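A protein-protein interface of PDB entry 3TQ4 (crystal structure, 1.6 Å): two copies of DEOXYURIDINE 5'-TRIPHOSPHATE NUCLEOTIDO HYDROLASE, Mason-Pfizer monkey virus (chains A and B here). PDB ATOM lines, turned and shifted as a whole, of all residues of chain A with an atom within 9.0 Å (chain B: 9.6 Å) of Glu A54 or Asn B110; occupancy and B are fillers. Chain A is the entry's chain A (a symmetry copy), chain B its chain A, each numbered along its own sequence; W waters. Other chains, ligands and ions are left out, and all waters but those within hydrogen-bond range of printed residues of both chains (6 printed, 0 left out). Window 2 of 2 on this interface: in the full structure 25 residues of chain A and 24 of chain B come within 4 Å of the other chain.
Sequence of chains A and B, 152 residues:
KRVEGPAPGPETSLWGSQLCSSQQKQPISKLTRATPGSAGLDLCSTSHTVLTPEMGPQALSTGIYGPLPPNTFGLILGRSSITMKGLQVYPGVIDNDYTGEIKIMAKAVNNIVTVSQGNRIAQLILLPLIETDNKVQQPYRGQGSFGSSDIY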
ATOM      1  N   VAL A  50      12.690  22.776   5.446  1.00  0.00           N
ATOM      2  CA  VAL A  50      11.852  21.798   6.144  1.00  0.00           C
ATOM      3  C   VAL A  50      10.793  22.564   6.929  1.00  0.00           C
ATOM      4  O   VAL A  50      11.138  23.563   7.589  1.00  0.00           O
ATOM      5  CB  VAL A  50      12.707  20.935   7.079  1.00  0.00           C
ATOM      6  CG1 VAL A  50      11.823  19.861   7.800  1.00  0.00           C
ATOM      7  CG2 VAL A  50      13.865  20.293   6.302  1.00  0.00           C
ATOM      8  N   LEU A  51       9.538  22.071   6.868  1.00  0.00           N
ATOM      9  CA  LEU A  51       8.363  22.683   7.547  1.00  0.00           C
ATOM     10  C   LEU A  51       7.670  21.641   8.427  1.00  0.00           C
ATOM     11  O   LEU A  51       7.488  20.507   8.013  1.00  0.00           O
ATOM     12  CB  LEU A  51       7.359  23.215   6.517  1.00  0.00           C
ATOM     13  CG  LEU A  51       7.781  24.298   5.524  1.00  0.00           C
ATOM     14  CD1 LEU A  51       6.514  24.663   4.766  1.00  0.00           C
ATOM     15  CD2 LEU A  51       8.384  25.537   6.230  1.00  0.00           C
ATOM     16  N   THR A  52       7.292  22.018   9.640  1.00  0.00           N
ATOM     17  CA  THR A  52       6.532  21.121  10.529  1.00  0.00           C
ATOM     18  C   THR A  52       5.270  21.892  10.902  1.00  0.00           C
ATOM     19  O   THR A  52       5.274  23.097  10.802  1.00  0.00           O
ATOM     20  CB  THR A  52       7.295  20.833  11.786  1.00  0.00           C
ATOM     21  OG1 THR A  52       7.640  22.059  12.400  1.00  0.00           O
ATOM     22  CG2 THR A  52       8.581  19.997  11.493  1.00  0.00           C
ATOM     23  N   PRO A  53       4.202  21.196  11.298  1.00  0.00           N
ATOM     24  CA  PRO A  53       2.934  21.890  11.663  1.00  0.00           C
ATOM     25  C   PRO A  53       3.143  22.949  12.750  1.00  0.00           C
ATOM     26  O   PRO A  53       2.613  24.065  12.633  1.00  0.00           O
ATOM     27  CB  PRO A  53       2.042  20.746  12.171  1.00  0.00           C
ATOM     28  CG  PRO A  53       2.636  19.494  11.451  1.00  0.00           C
ATOM     29  CD  PRO A  53       4.106  19.732  11.395  1.00  0.00           C
ATOM     30  N   GLU A  54       3.949  22.649  13.760  1.00  0.00           N
ATOM     31  CA  GLU A  54       4.079  23.620  14.853  1.00  0.00           C
ATOM     32  C   GLU A  54       4.756  24.891  14.440  1.00  0.00           C
ATOM     33  O   GLU A  54       4.685  25.882  15.182  1.00  0.00           O
ATOM     34  CB  GLU A  54       4.719  23.020  16.123  1.00  0.00           C
ATOM     35  CG  GLU A  54       6.158  22.723  15.940  1.00  0.00           C
ATOM     36  CD  GLU A  54       6.463  21.380  15.267  1.00  0.00           C
ATOM     37  OE1 GLU A  54       5.530  20.612  14.808  1.00  0.00           O
ATOM     38  OE2 GLU A  54       7.710  21.098  15.226  1.00  0.00           O
ATOM     39  N   MET A  55       5.390  24.928  13.270  1.00  0.00           N
ATOM     40  CA  MET A  55       6.063  26.154  12.856  1.00  0.00           C
ATOM     41  C   MET A  55       5.091  27.237  12.376  1.00  0.00           C
ATOM     42  O   MET A  55       5.444  28.438  12.349  1.00  0.00           O
ATOM     43  CB  MET A  55       7.102  25.873  11.764  1.00  0.00           C
ATOM     44  CG  MET A  55       8.377  25.359  12.278  1.00  0.00           C
ATOM     45  SD  MET A  55       9.267  24.736  10.799  1.00  0.00           S
ATOM     46  CE  MET A  55       9.695  26.192   9.946  1.00  0.00           C
ATOM     47  N   GLY A  56       3.872  26.844  12.020  1.00  0.00           N
ATOM     48  CA  GLY A  56       2.938  27.834  11.447  1.00  0.00           C
ATOM     49  C   GLY A  56       3.404  28.413  10.106  1.00  0.00           C
ATOM     50  O   GLY A  56       4.379  27.918   9.500  1.00  0.00           O
ATOM     51  N   PRO A  57       2.705  29.459   9.627  1.00  0.00           N
ATOM     52  CA  PRO A  57       2.958  29.956   8.255  1.00  0.00           C
ATOM     53  C   PRO A  57       4.412  30.385   8.045  1.00  0.00           C
ATOM     54  O   PRO A  57       5.008  31.077   8.892  1.00  0.00           O
ATOM     55  CB  PRO A  57       1.976  31.137   8.144  1.00  0.00           C
ATOM     56  CG  PRO A  57       0.839  30.745   9.086  1.00  0.00           C
ATOM     57  CD  PRO A  57       1.604  30.196  10.283  1.00  0.00           C
ATOM     58  N   GLN A  58       4.981  29.986   6.918  1.00  0.00           N
ATOM     59  CA  GLN A  58       6.314  30.416   6.573  1.00  0.00           C
ATOM     60  C   GLN A  58       6.329  31.070   5.210  1.00  0.00           C
ATOM     61  O   GLN A  58       5.646  30.589   4.307  1.00  0.00           O
ATOM     62  CB  GLN A  58       7.226  29.195   6.525  1.00  0.00           C
ATOM     63  CG  GLN A  58       7.402  28.486   7.862  1.00  0.00           C
ATOM     64  CD  GLN A  58       8.149  29.282   8.845  1.00  0.00           C
ATOM     65  OE1 GLN A  58       9.275  29.679   8.583  1.00  0.00           O
ATOM     66  NE2 GLN A  58       7.565  29.483  10.034  1.00  0.00           N
ATOM     67  N   TYR A  90      -1.281  29.318   1.496  1.00  0.00           N
ATOM     68  CA  TYR A  90      -2.352  30.247   1.813  1.00  0.00           C
ATOM     69  C   TYR A  90      -2.515  31.166   0.586  1.00  0.00           C
ATOM     70  O   TYR A  90      -1.541  31.735   0.141  1.00  0.00           O
ATOM     71  CB  TYR A  90      -1.988  31.120   3.010  1.00  0.00           C
ATOM     72  CG  TYR A  90      -1.863  30.332   4.286  1.00  0.00           C
ATOM     73  CD1 TYR A  90      -2.975  29.796   4.888  1.00  0.00           C
ATOM     74  CD2 TYR A  90      -0.590  30.017   4.820  1.00  0.00           C
ATOM     75  CE1 TYR A  90      -2.863  29.023   6.069  1.00  0.00           C
ATOM     76  CE2 TYR A  90      -0.467  29.241   6.027  1.00  0.00           C
ATOM     77  CZ  TYR A  90      -1.628  28.757   6.631  1.00  0.00           C
ATOM     78  OH  TYR A  90      -1.595  28.010   7.806  1.00  0.00           O
ATOM     79  N   LYS A 107       2.308  26.205   4.901  1.00  0.00           N
ATOM     80  CA  LYS A 107       2.342  25.575   6.216  1.00  0.00           C
ATOM     81  C   LYS A 107       2.254  24.078   6.031  1.00  0.00           C
ATOM     82  O   LYS A 107       1.443  23.613   5.244  1.00  0.00           O
ATOM     83  CB  LYS A 107       1.127  26.042   7.057  1.00  0.00           C
ATOM     84  CG  LYS A 107       1.237  25.578   8.554  1.00  0.00           C
ATOM     85  CD  LYS A 107       0.012  25.640   9.341  1.00  0.00           C
ATOM     86  CE  LYS A 107       0.166  24.745  10.580  1.00  0.00           C
ATOM     87  NZ  LYS A 107      -0.544  23.372  10.452  1.00  0.00           N
ATOM     88  N   ALA A 108       3.063  23.300   6.760  1.00  0.00           N
ATOM     89  CA  ALA A 108       2.871  21.849   6.795  1.00  0.00           C
ATOM     90  C   ALA A 108       1.597  21.538   7.586  1.00  0.00           C
ATOM     91  O   ALA A 108       1.432  21.991   8.717  1.00  0.00           O
ATOM     92  CB  ALA A 108       4.076  21.143   7.428  1.00  0.00           C
ATOM     93  N   VAL A 109       0.698  20.760   6.966  1.00  0.00           N
ATOM     94  CA  VAL A 109      -0.635  20.519   7.541  1.00  0.00           C
ATOM     95  C   VAL A 109      -0.586  19.587   8.785  1.00  0.00           C
ATOM     96  O   VAL A 109      -1.065  19.968   9.888  1.00  0.00           O
ATOM     97  CB  VAL A 109      -1.585  19.946   6.429  1.00  0.00           C
ATOM     98  CG1 VAL A 109      -2.881  19.400   7.008  1.00  0.00           C
ATOM     99  CG2 VAL A 109      -1.818  20.997   5.319  1.00  0.00           C
ATOM    100  N   ASN A 110      -0.027  18.392   8.581  1.00  0.00           N
ATOM    101  CA  ASN A 110      -0.044  17.348   9.586  1.00  0.00           C
ATOM    102  C   ASN A 110       1.307  16.725   9.858  1.00  0.00           C
ATOM    103  O   ASN A 110       1.537  16.207  10.967  1.00  0.00           O
ATOM    104  CB  ASN A 110      -1.039  16.237   9.171  1.00  0.00           C
ATOM    105  CG  ASN A 110      -2.383  16.395   9.825  1.00  0.00           C
ATOM    106  OD1 ASN A 110      -2.557  17.194  10.755  1.00  0.00           O
ATOM    107  ND2 ASN A 110      -3.343  15.618   9.372  1.00  0.00           N
ATOM    108  N   ASN A 111       2.180  16.778   8.866  1.00  0.00           N
ATOM    109  CA  ASN A 111       3.414  16.036   8.870  1.00  0.00           C
ATOM    110  C   ASN A 111       4.573  16.910   8.509  1.00  0.00           C
ATOM    111  O   ASN A 111       4.372  18.020   8.047  1.00  0.00           O
ATOM    112  CB  ASN A 111       3.322  14.936   7.812  1.00  0.00           C
ATOM    113  CG  ASN A 111       1.964  14.148   7.873  1.00  0.00           C
ATOM    114  OD1 ASN A 111       1.245  14.012   6.871  1.00  0.00           O
ATOM    115  ND2 ASN A 111       1.621  13.670   9.057  1.00  0.00           N
ATOM    116  N   ILE A 112       5.770  16.352   8.645  1.00  0.00           N
ATOM    117  CA  ILE A 112       7.019  17.016   8.240  1.00  0.00           C
ATOM    118  C   ILE A 112       7.085  17.047   6.717  1.00  0.00           C
ATOM    119  O   ILE A 112       6.897  16.017   6.081  1.00  0.00           O
ATOM    120  CB  ILE A 112       8.218  16.256   8.768  1.00  0.00           C
ATOM    121  CG1 ILE A 112       8.153  16.223  10.297  1.00  0.00           C
ATOM    122  CG2 ILE A 112       9.471  16.882   8.230  1.00  0.00           C
ATOM    123  CD1 ILE A 112       9.165  15.317  10.941  1.00  0.00           C
ATOM    124  N   LEU B  51      -9.113  34.387  19.518  1.00  0.00           N
ATOM    125  CA  LEU B  51      -9.268  33.108  18.774  1.00  0.00           C
ATOM    126  C   LEU B  51      -8.167  32.129  19.188  1.00  0.00           C
ATOM    127  O   LEU B  51      -7.015  32.513  19.310  1.00  0.00           O
ATOM    128  CB  LEU B  51      -9.181  33.347  17.261  1.00  0.00           C
ATOM    129  CG  LEU B  51     -10.190  34.267  16.572  1.00  0.00           C
ATOM    130  CD1 LEU B  51      -9.882  34.160  15.087  1.00  0.00           C
ATOM    131  CD2 LEU B  51     -11.654  33.858  16.869  1.00  0.00           C
ATOM    132  N   THR B  52      -8.518  30.871  19.410  1.00  0.00           N
ATOM    133  CA  THR B  52      -7.521  29.831  19.718  1.00  0.00           C
ATOM    134  C   THR B  52      -7.738  28.738  18.676  1.00  0.00           C
ATOM    135  O   THR B  52      -8.808  28.673  18.117  1.00  0.00           O
ATOM    136  CB  THR B  52      -7.758  29.240  21.075  1.00  0.00           C
ATOM    137  OG1 THR B  52      -9.089  28.768  21.139  1.00  0.00           O
ATOM    138  CG2 THR B  52      -7.503  30.288  22.204  1.00  0.00           C
ATOM    139  N   PRO B  53      -6.724  27.914  18.409  1.00  0.00           N
ATOM    140  CA  PRO B  53      -6.867  26.832  17.392  1.00  0.00           C
ATOM    141  C   PRO B  53      -8.059  25.915  17.684  1.00  0.00           C
ATOM    142  O   PRO B  53      -8.823  25.585  16.764  1.00  0.00           O
ATOM    143  CB  PRO B  53      -5.541  26.067  17.503  1.00  0.00           C
ATOM    144  CG  PRO B  53      -4.563  27.143  18.074  1.00  0.00           C
ATOM    145  CD  PRO B  53      -5.383  27.961  19.011  1.00  0.00           C
ATOM    146  N   GLU B  54      -8.269  25.554  18.944  1.00  0.00           N
ATOM    147  CA  GLU B  54      -9.349  24.598  19.218  1.00  0.00           C
ATOM    148  C   GLU B  54     -10.714  25.153  18.950  1.00  0.00           C
ATOM    149  O   GLU B  54     -11.678  24.377  18.881  1.00  0.00           O
ATOM    150  CB  GLU B  54      -9.256  23.970  20.625  1.00  0.00           C
ATOM    151  CG  GLU B  54      -9.564  24.943  21.698  1.00  0.00           C
ATOM    152  CD  GLU B  54      -8.391  25.834  22.123  1.00  0.00           C
ATOM    153  OE1 GLU B  54      -7.248  25.800  21.522  1.00  0.00           O
ATOM    154  OE2 GLU B  54      -8.653  26.582  23.127  1.00  0.00           O
ATOM    155  N   THR B  83      -1.990  36.776   7.841  1.00  0.00           N
ATOM    156  CA  THR B  83      -1.708  35.348   7.676  1.00  0.00           C
ATOM    157  C   THR B  83      -0.371  34.918   8.341  1.00  0.00           C
ATOM    158  O   THR B  83      -0.280  33.884   9.039  1.00  0.00           O
ATOM    159  CB  THR B  83      -1.675  34.967   6.193  1.00  0.00           C
ATOM    160  OG1 THR B  83      -2.927  35.350   5.626  1.00  0.00           O
ATOM    161  CG2 THR B  83      -1.394  33.429   5.998  1.00  0.00           C
ATOM    162  N   MET B  84       0.665  35.732   8.182  1.00  0.00           N
ATOM    163  CA  MET B  84       1.987  35.387   8.692  1.00  0.00           C
ATOM    164  C   MET B  84       2.071  35.531  10.213  1.00  0.00           C
ATOM    165  O   MET B  84       2.981  34.964  10.843  1.00  0.00           O
ATOM    166  CB  MET B  84       3.020  36.277   8.023  1.00  0.00           C
ATOM    167  CG  MET B  84       3.232  35.959   6.535  1.00  0.00           C
ATOM    168  SD  MET B  84       3.788  34.272   6.243  1.00  0.00           S
ATOM    169  CE  MET B  84       5.302  34.177   7.204  1.00  0.00           C
ATOM    170  N   LYS B  85       1.150  36.297  10.790  1.00  0.00           N
ATOM    171  CA  LYS B  85       0.984  36.396  12.232  1.00  0.00           C
ATOM    172  C   LYS B  85       0.056  35.314  12.819  1.00  0.00           C
ATOM    173  O   LYS B  85      -0.226  35.328  14.028  1.00  0.00           O
ATOM    174  CB  LYS B  85       0.468  37.786  12.626  1.00  0.00           C
ATOM    175  CG  LYS B  85       1.505  38.892  12.443  1.00  0.00           C
ATOM    176  CD  LYS B  85       0.863  40.192  12.799  1.00  0.00           C
ATOM    177  CE  LYS B  85       1.862  41.336  12.855  1.00  0.00           C
ATOM    178  NZ  LYS B  85       2.048  41.964  11.505  1.00  0.00           N
ATOM    179  N   GLY B  86      -0.413  34.385  12.006  1.00  0.00           N
ATOM    180  CA  GLY B  86      -1.023  33.190  12.537  1.00  0.00           C
ATOM    181  C   GLY B  86      -2.541  33.150  12.487  1.00  0.00           C
ATOM    182  O   GLY B  86      -3.164  32.214  13.055  1.00  0.00           O
ATOM    183  N   LEU B  87      -3.151  34.104  11.780  1.00  0.00           N
ATOM    184  CA  LEU B  87      -4.610  34.111  11.619  1.00  0.00           C
ATOM    185  C   LEU B  87      -4.951  33.813  10.183  1.00  0.00           C
ATOM    186  O   LEU B  87      -4.621  34.610   9.263  1.00  0.00           O
ATOM    187  CB  LEU B  87      -5.187  35.458  12.031  1.00  0.00           C
ATOM    188  CG  LEU B  87      -6.713  35.586  11.903  1.00  0.00           C
ATOM    189  CD1 LEU B  87      -7.426  34.558  12.801  1.00  0.00           C
ATOM    190  CD2 LEU B  87      -7.127  37.016  12.284  1.00  0.00           C
ATOM    191  N   GLN B  88      -5.571  32.658   9.978  1.00  0.00           N
ATOM    192  CA  GLN B  88      -5.952  32.243   8.637  1.00  0.00           C
ATOM    193  C   GLN B  88      -7.355  32.734   8.318  1.00  0.00           C
ATOM    194  O   GLN B  88      -8.295  32.550   9.101  1.00  0.00           O
ATOM    195  CB  GLN B  88      -5.927  30.727   8.544  1.00  0.00           C
ATOM    196  CG  GLN B  88      -6.613  30.220   7.284  1.00  0.00           C
ATOM    197  CD  GLN B  88      -6.538  28.732   7.153  1.00  0.00           C
ATOM    198  OE1 GLN B  88      -6.361  27.987   8.125  1.00  0.00           O
ATOM    199  NE2 GLN B  88      -6.673  28.279   5.949  1.00  0.00           N
ATOM    200  N   LYS B 107      -9.529  31.562  11.452  1.00  0.00           N
ATOM    201  CA  LYS B 107      -9.163  30.569  12.455  1.00  0.00           C
ATOM    202  C   LYS B 107      -7.755  30.859  12.923  1.00  0.00           C
ATOM    203  O   LYS B 107      -6.889  31.127  12.105  1.00  0.00           O
ATOM    204  CB  LYS B 107      -9.194  29.151  11.830  1.00  0.00           C
ATOM    205  CG  LYS B 107      -9.034  28.028  12.916  1.00  0.00           C
ATOM    206  CD  LYS B 107      -8.688  26.699  12.425  1.00  0.00           C
ATOM    207  CE  LYS B 107      -8.123  25.867  13.586  1.00  0.00           C
ATOM    208  NZ  LYS B 107      -6.576  25.756  13.582  1.00  0.00           N
ATOM    209  N   ALA B 108      -7.498  30.793  14.235  1.00  0.00           N
ATOM    210  CA  ALA B 108      -6.121  30.839  14.728  1.00  0.00           C
ATOM    211  C   ALA B 108      -5.421  29.527  14.362  1.00  0.00           C
ATOM    212  O   ALA B 108      -5.918  28.443  14.662  1.00  0.00           O
ATOM    213  CB  ALA B 108      -6.079  31.058  16.245  1.00  0.00           C
ATOM    214  N   VAL B 109      -4.259  29.647  13.702  1.00  0.00           N
ATOM    215  CA  VAL B 109      -3.568  28.473  13.147  1.00  0.00           C
ATOM    216  C   VAL B 109      -2.926  27.583  14.250  1.00  0.00           C
ATOM    217  O   VAL B 109      -3.224  26.360  14.338  1.00  0.00           O
ATOM    218  CB  VAL B 109      -2.500  28.947  12.097  1.00  0.00           C
ATOM    219  CG1 VAL B 109      -1.550  27.827  11.699  1.00  0.00           C
ATOM    220  CG2 VAL B 109      -3.189  29.609  10.881  1.00  0.00           C
ATOM    221  N   ASN B 110      -2.058  28.206  15.050  1.00  0.00           N
ATOM    222  CA  ASN B 110      -1.255  27.492  16.024  1.00  0.00           C
ATOM    223  C   ASN B 110      -1.299  28.080  17.416  1.00  0.00           C
ATOM    224  O   ASN B 110      -1.086  27.351  18.403  1.00  0.00           O
ATOM    225  CB  ASN B 110       0.216  27.431  15.546  1.00  0.00           C
ATOM    226  CG  ASN B 110       0.544  26.136  14.857  1.00  0.00           C
ATOM    227  OD1 ASN B 110      -0.232  25.172  14.896  1.00  0.00           O
ATOM    228  ND2 ASN B 110       1.705  26.085  14.242  1.00  0.00           N
ATOM    229  N   ASN B 111      -1.571  29.372  17.492  1.00  0.00           N
ATOM    230  CA  ASN B 111      -1.421  30.134  18.704  1.00  0.00           C
ATOM    231  C   ASN B 111      -2.638  30.957  18.981  1.00  0.00           C
ATOM    232  O   ASN B 111      -3.486  31.094  18.116  1.00  0.00           O
ATOM    233  CB  ASN B 111      -0.245  31.098  18.529  1.00  0.00           C
ATOM    234  CG  ASN B 111       1.020  30.403  17.909  1.00  0.00           C
ATOM    235  OD1 ASN B 111       1.583  30.858  16.901  1.00  0.00           O
ATOM    236  ND2 ASN B 111       1.425  29.295  18.503  1.00  0.00           N
ATOM    237  N   ILE B 112      -2.657  31.567  20.160  1.00  0.00           N
ATOM    238  CA  ILE B 112      -3.717  32.501  20.568  1.00  0.00           C
ATOM    239  C   ILE B 112      -3.558  33.797  19.779  1.00  0.00           C
ATOM    240  O   ILE B 112      -2.466  34.349  19.734  1.00  0.00           O
ATOM    241  CB  ILE B 112      -3.610  32.812  22.047  1.00  0.00           C
ATOM    242  CG1 ILE B 112      -3.769  31.514  22.842  1.00  0.00           C
ATOM    243  CG2 ILE B 112      -4.620  33.864  22.402  1.00  0.00           C
ATOM    244  CD1 ILE B 112      -3.468  31.644  24.308  1.00  0.00           C
ATOM    245  N   VAL B 113      -4.623  34.231  19.111  1.00  0.00           N
ATOM    246  CA  VAL B 113      -4.623  35.445  18.270  1.00  0.00           C
ATOM    247  C   VAL B 113      -5.639  36.408  18.870  1.00  0.00           C
ATOM    248  O   VAL B 113      -6.749  36.000  19.208  1.00  0.00           O
ATOM    249  CB  VAL B 113      -4.990  35.109  16.764  1.00  0.00           C
ATOM    250  CG1 VAL B 113      -5.171  36.398  15.950  1.00  0.00           C
ATOM    251  CG2 VAL B 113      -3.935  34.220  16.147  1.00  0.00           C
HETATM  252  O   HOH W   1      -3.531  26.513   8.193  1.00  0.00           O
HETATM  253  O   HOH W   2       3.968  29.017  15.895  1.00  0.00           O
HETATM  254  O   HOH W   3       0.936  22.019  15.264  1.00  0.00           O
HETATM  255  O   HOH W   4      -0.784  22.704  13.511  1.00  0.00           O
HETATM  256  O   HOH W   5       4.277  32.491  10.874  1.00  0.00           O
HETATM  257  O   HOH W   6       3.205  26.509  17.423  1.00  0.00           O
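ND2 of Asn B110 lies within hydrogen-bond range of O of Pro A53 (2.7 Å). ND2 of Asn B110 lies within hydrogen-bond range of O of Glu A54. N of Gly A56 sits close to ND2 of Asn B110 (3.2 Å).
The backbone carbonyl oxygen (O) of Gly B86 lies within hydrogen-bond range of the backbone NH (N) of Val B109. The backbone NH (N) of Lys B107 is in hydrogen-bond range of the backbone carbonyl oxygen (O) of Gln B88, at 2.8 Å. The side-chain amino group of Lys B107 lies within hydrogen-bond range of the backbone carbonyl oxygen of Val B109. The side-chain carboxylate (OE2) of Glu A54 is in hydrogen-bond range of the side-chain hydroxyl (OG1) of Thr A52 (3.0 Å). The side-chain sulfur (SD) of Met A55 sits close to the side-chain hydroxyl (OG1) of Thr A52. O of Met A55 sits at hydrogen-bond distance from NE2 of Gln A58, 3.3 Å away.
Among the printed residues, merely in contact across the chains: Pro A57 with Thr B83 (3.3 Å), Pro A57 with Met B84 (3.5 Å), Tyr A90 with Thr B83 (3.6 Å), Lys A107 with Val B109 (3.6 Å), Tyr A90 with Val B109 (3.8 Å), Gln A58 with Met B84 (3.8 Å), Tyr A90 with Gln B88 (3.8 Å) and Met A55 with Asn B110 (3.98 Å).
Of the printed residues of chain B, Glu A54 touches Asn B110. Printed residues of chain A within 4 Å of Asn B110: Pro A53 (2.7 Å), Glu A54 (3.1 Å), Met A55 (3.98 Å) and Gly A56 (3.2 Å). Thr A52 touches none of the printed residues of chain B. No residue of chain A comes within 4 Å of Asn B111. Of the printed residues of chain B, Met A55 touches Asn B110. Of the printed residues of chain A, Gln B88 touches Tyr A90 (3.8 Å). Of the printed residues of chain B, Gln A58 touches Met B84. Printed residues of chain B within 4 Å of Tyr A90: Thr B83, Gln B88 and Val B109. Of the printed residues of chain A, Thr B83 touches Pro A57 (3.3 Å) and Tyr A90 (3.6 Å). Pro B53 touches none of the printed residues of chain A. The nearest printed residue of chain A that does not touch Asn B110 is Lys A107 (4.2 Å). The nearest printed residue of chain B that does not touch Gly A56 is Val B109 (4.5 Å).
Hydrophobic or aromatic side chains of chain B within 4 Å of the printed part of chain A: Met B84 and Val B109. Along chain B the printed residues that touch a printed residue of chain A span positions 83 to 110. Hydrophobic or aromatic side chains of chain A within 4 Å of the printed part of chain B: Pro A57 and Tyr A90. Among the printed residues, 11 pairs touch across the chains. Among the printed residues, no Asp or Glu carboxylate lies within 4 Å of a Lys or Arg side-chain nitrogen of the other chain.
Pro A53 touches Asn B110, but with the chains exchanged Asn A110 does not touch Pro B53 (11.5 Å). Glu A54 touches Asn B110, but with the chains exchanged Asn A110 does not touch Glu B54 (13.0 Å). Lys A107 touches Val B109, but with the chains exchanged Val A109 does not touch Lys B107 (8.8 Å). Positions printed for both chains: 51, 52, 53, 54, 107, 108, 109, 110, 111 and 112.
Water W1 bridges OH of Tyr A90 and OE1 of Gln B88. Water W5 bridges the backbone carbonyl oxygen of Pro A57 and the backbone carbonyl oxygen of Met B84. Water W6 bridges O of Glu A54 (2.8 Å) and ND2 of Asn B111 (3.5 Å). Water W4 bridges the side-chain amide oxygen of Asn B110 and the side-chain amino group of Lys A107. Water W2 bridges OD1 of Asn B111 (3.2 Å) and O of Glu A54 (3.3 Å). Water W3 lies within hydrogen-bond range of the side-chain amide oxygen (OD1) of Asn B110 (3.4 Å) and the backbone NH (N) of Glu A54 (3.4 Å).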
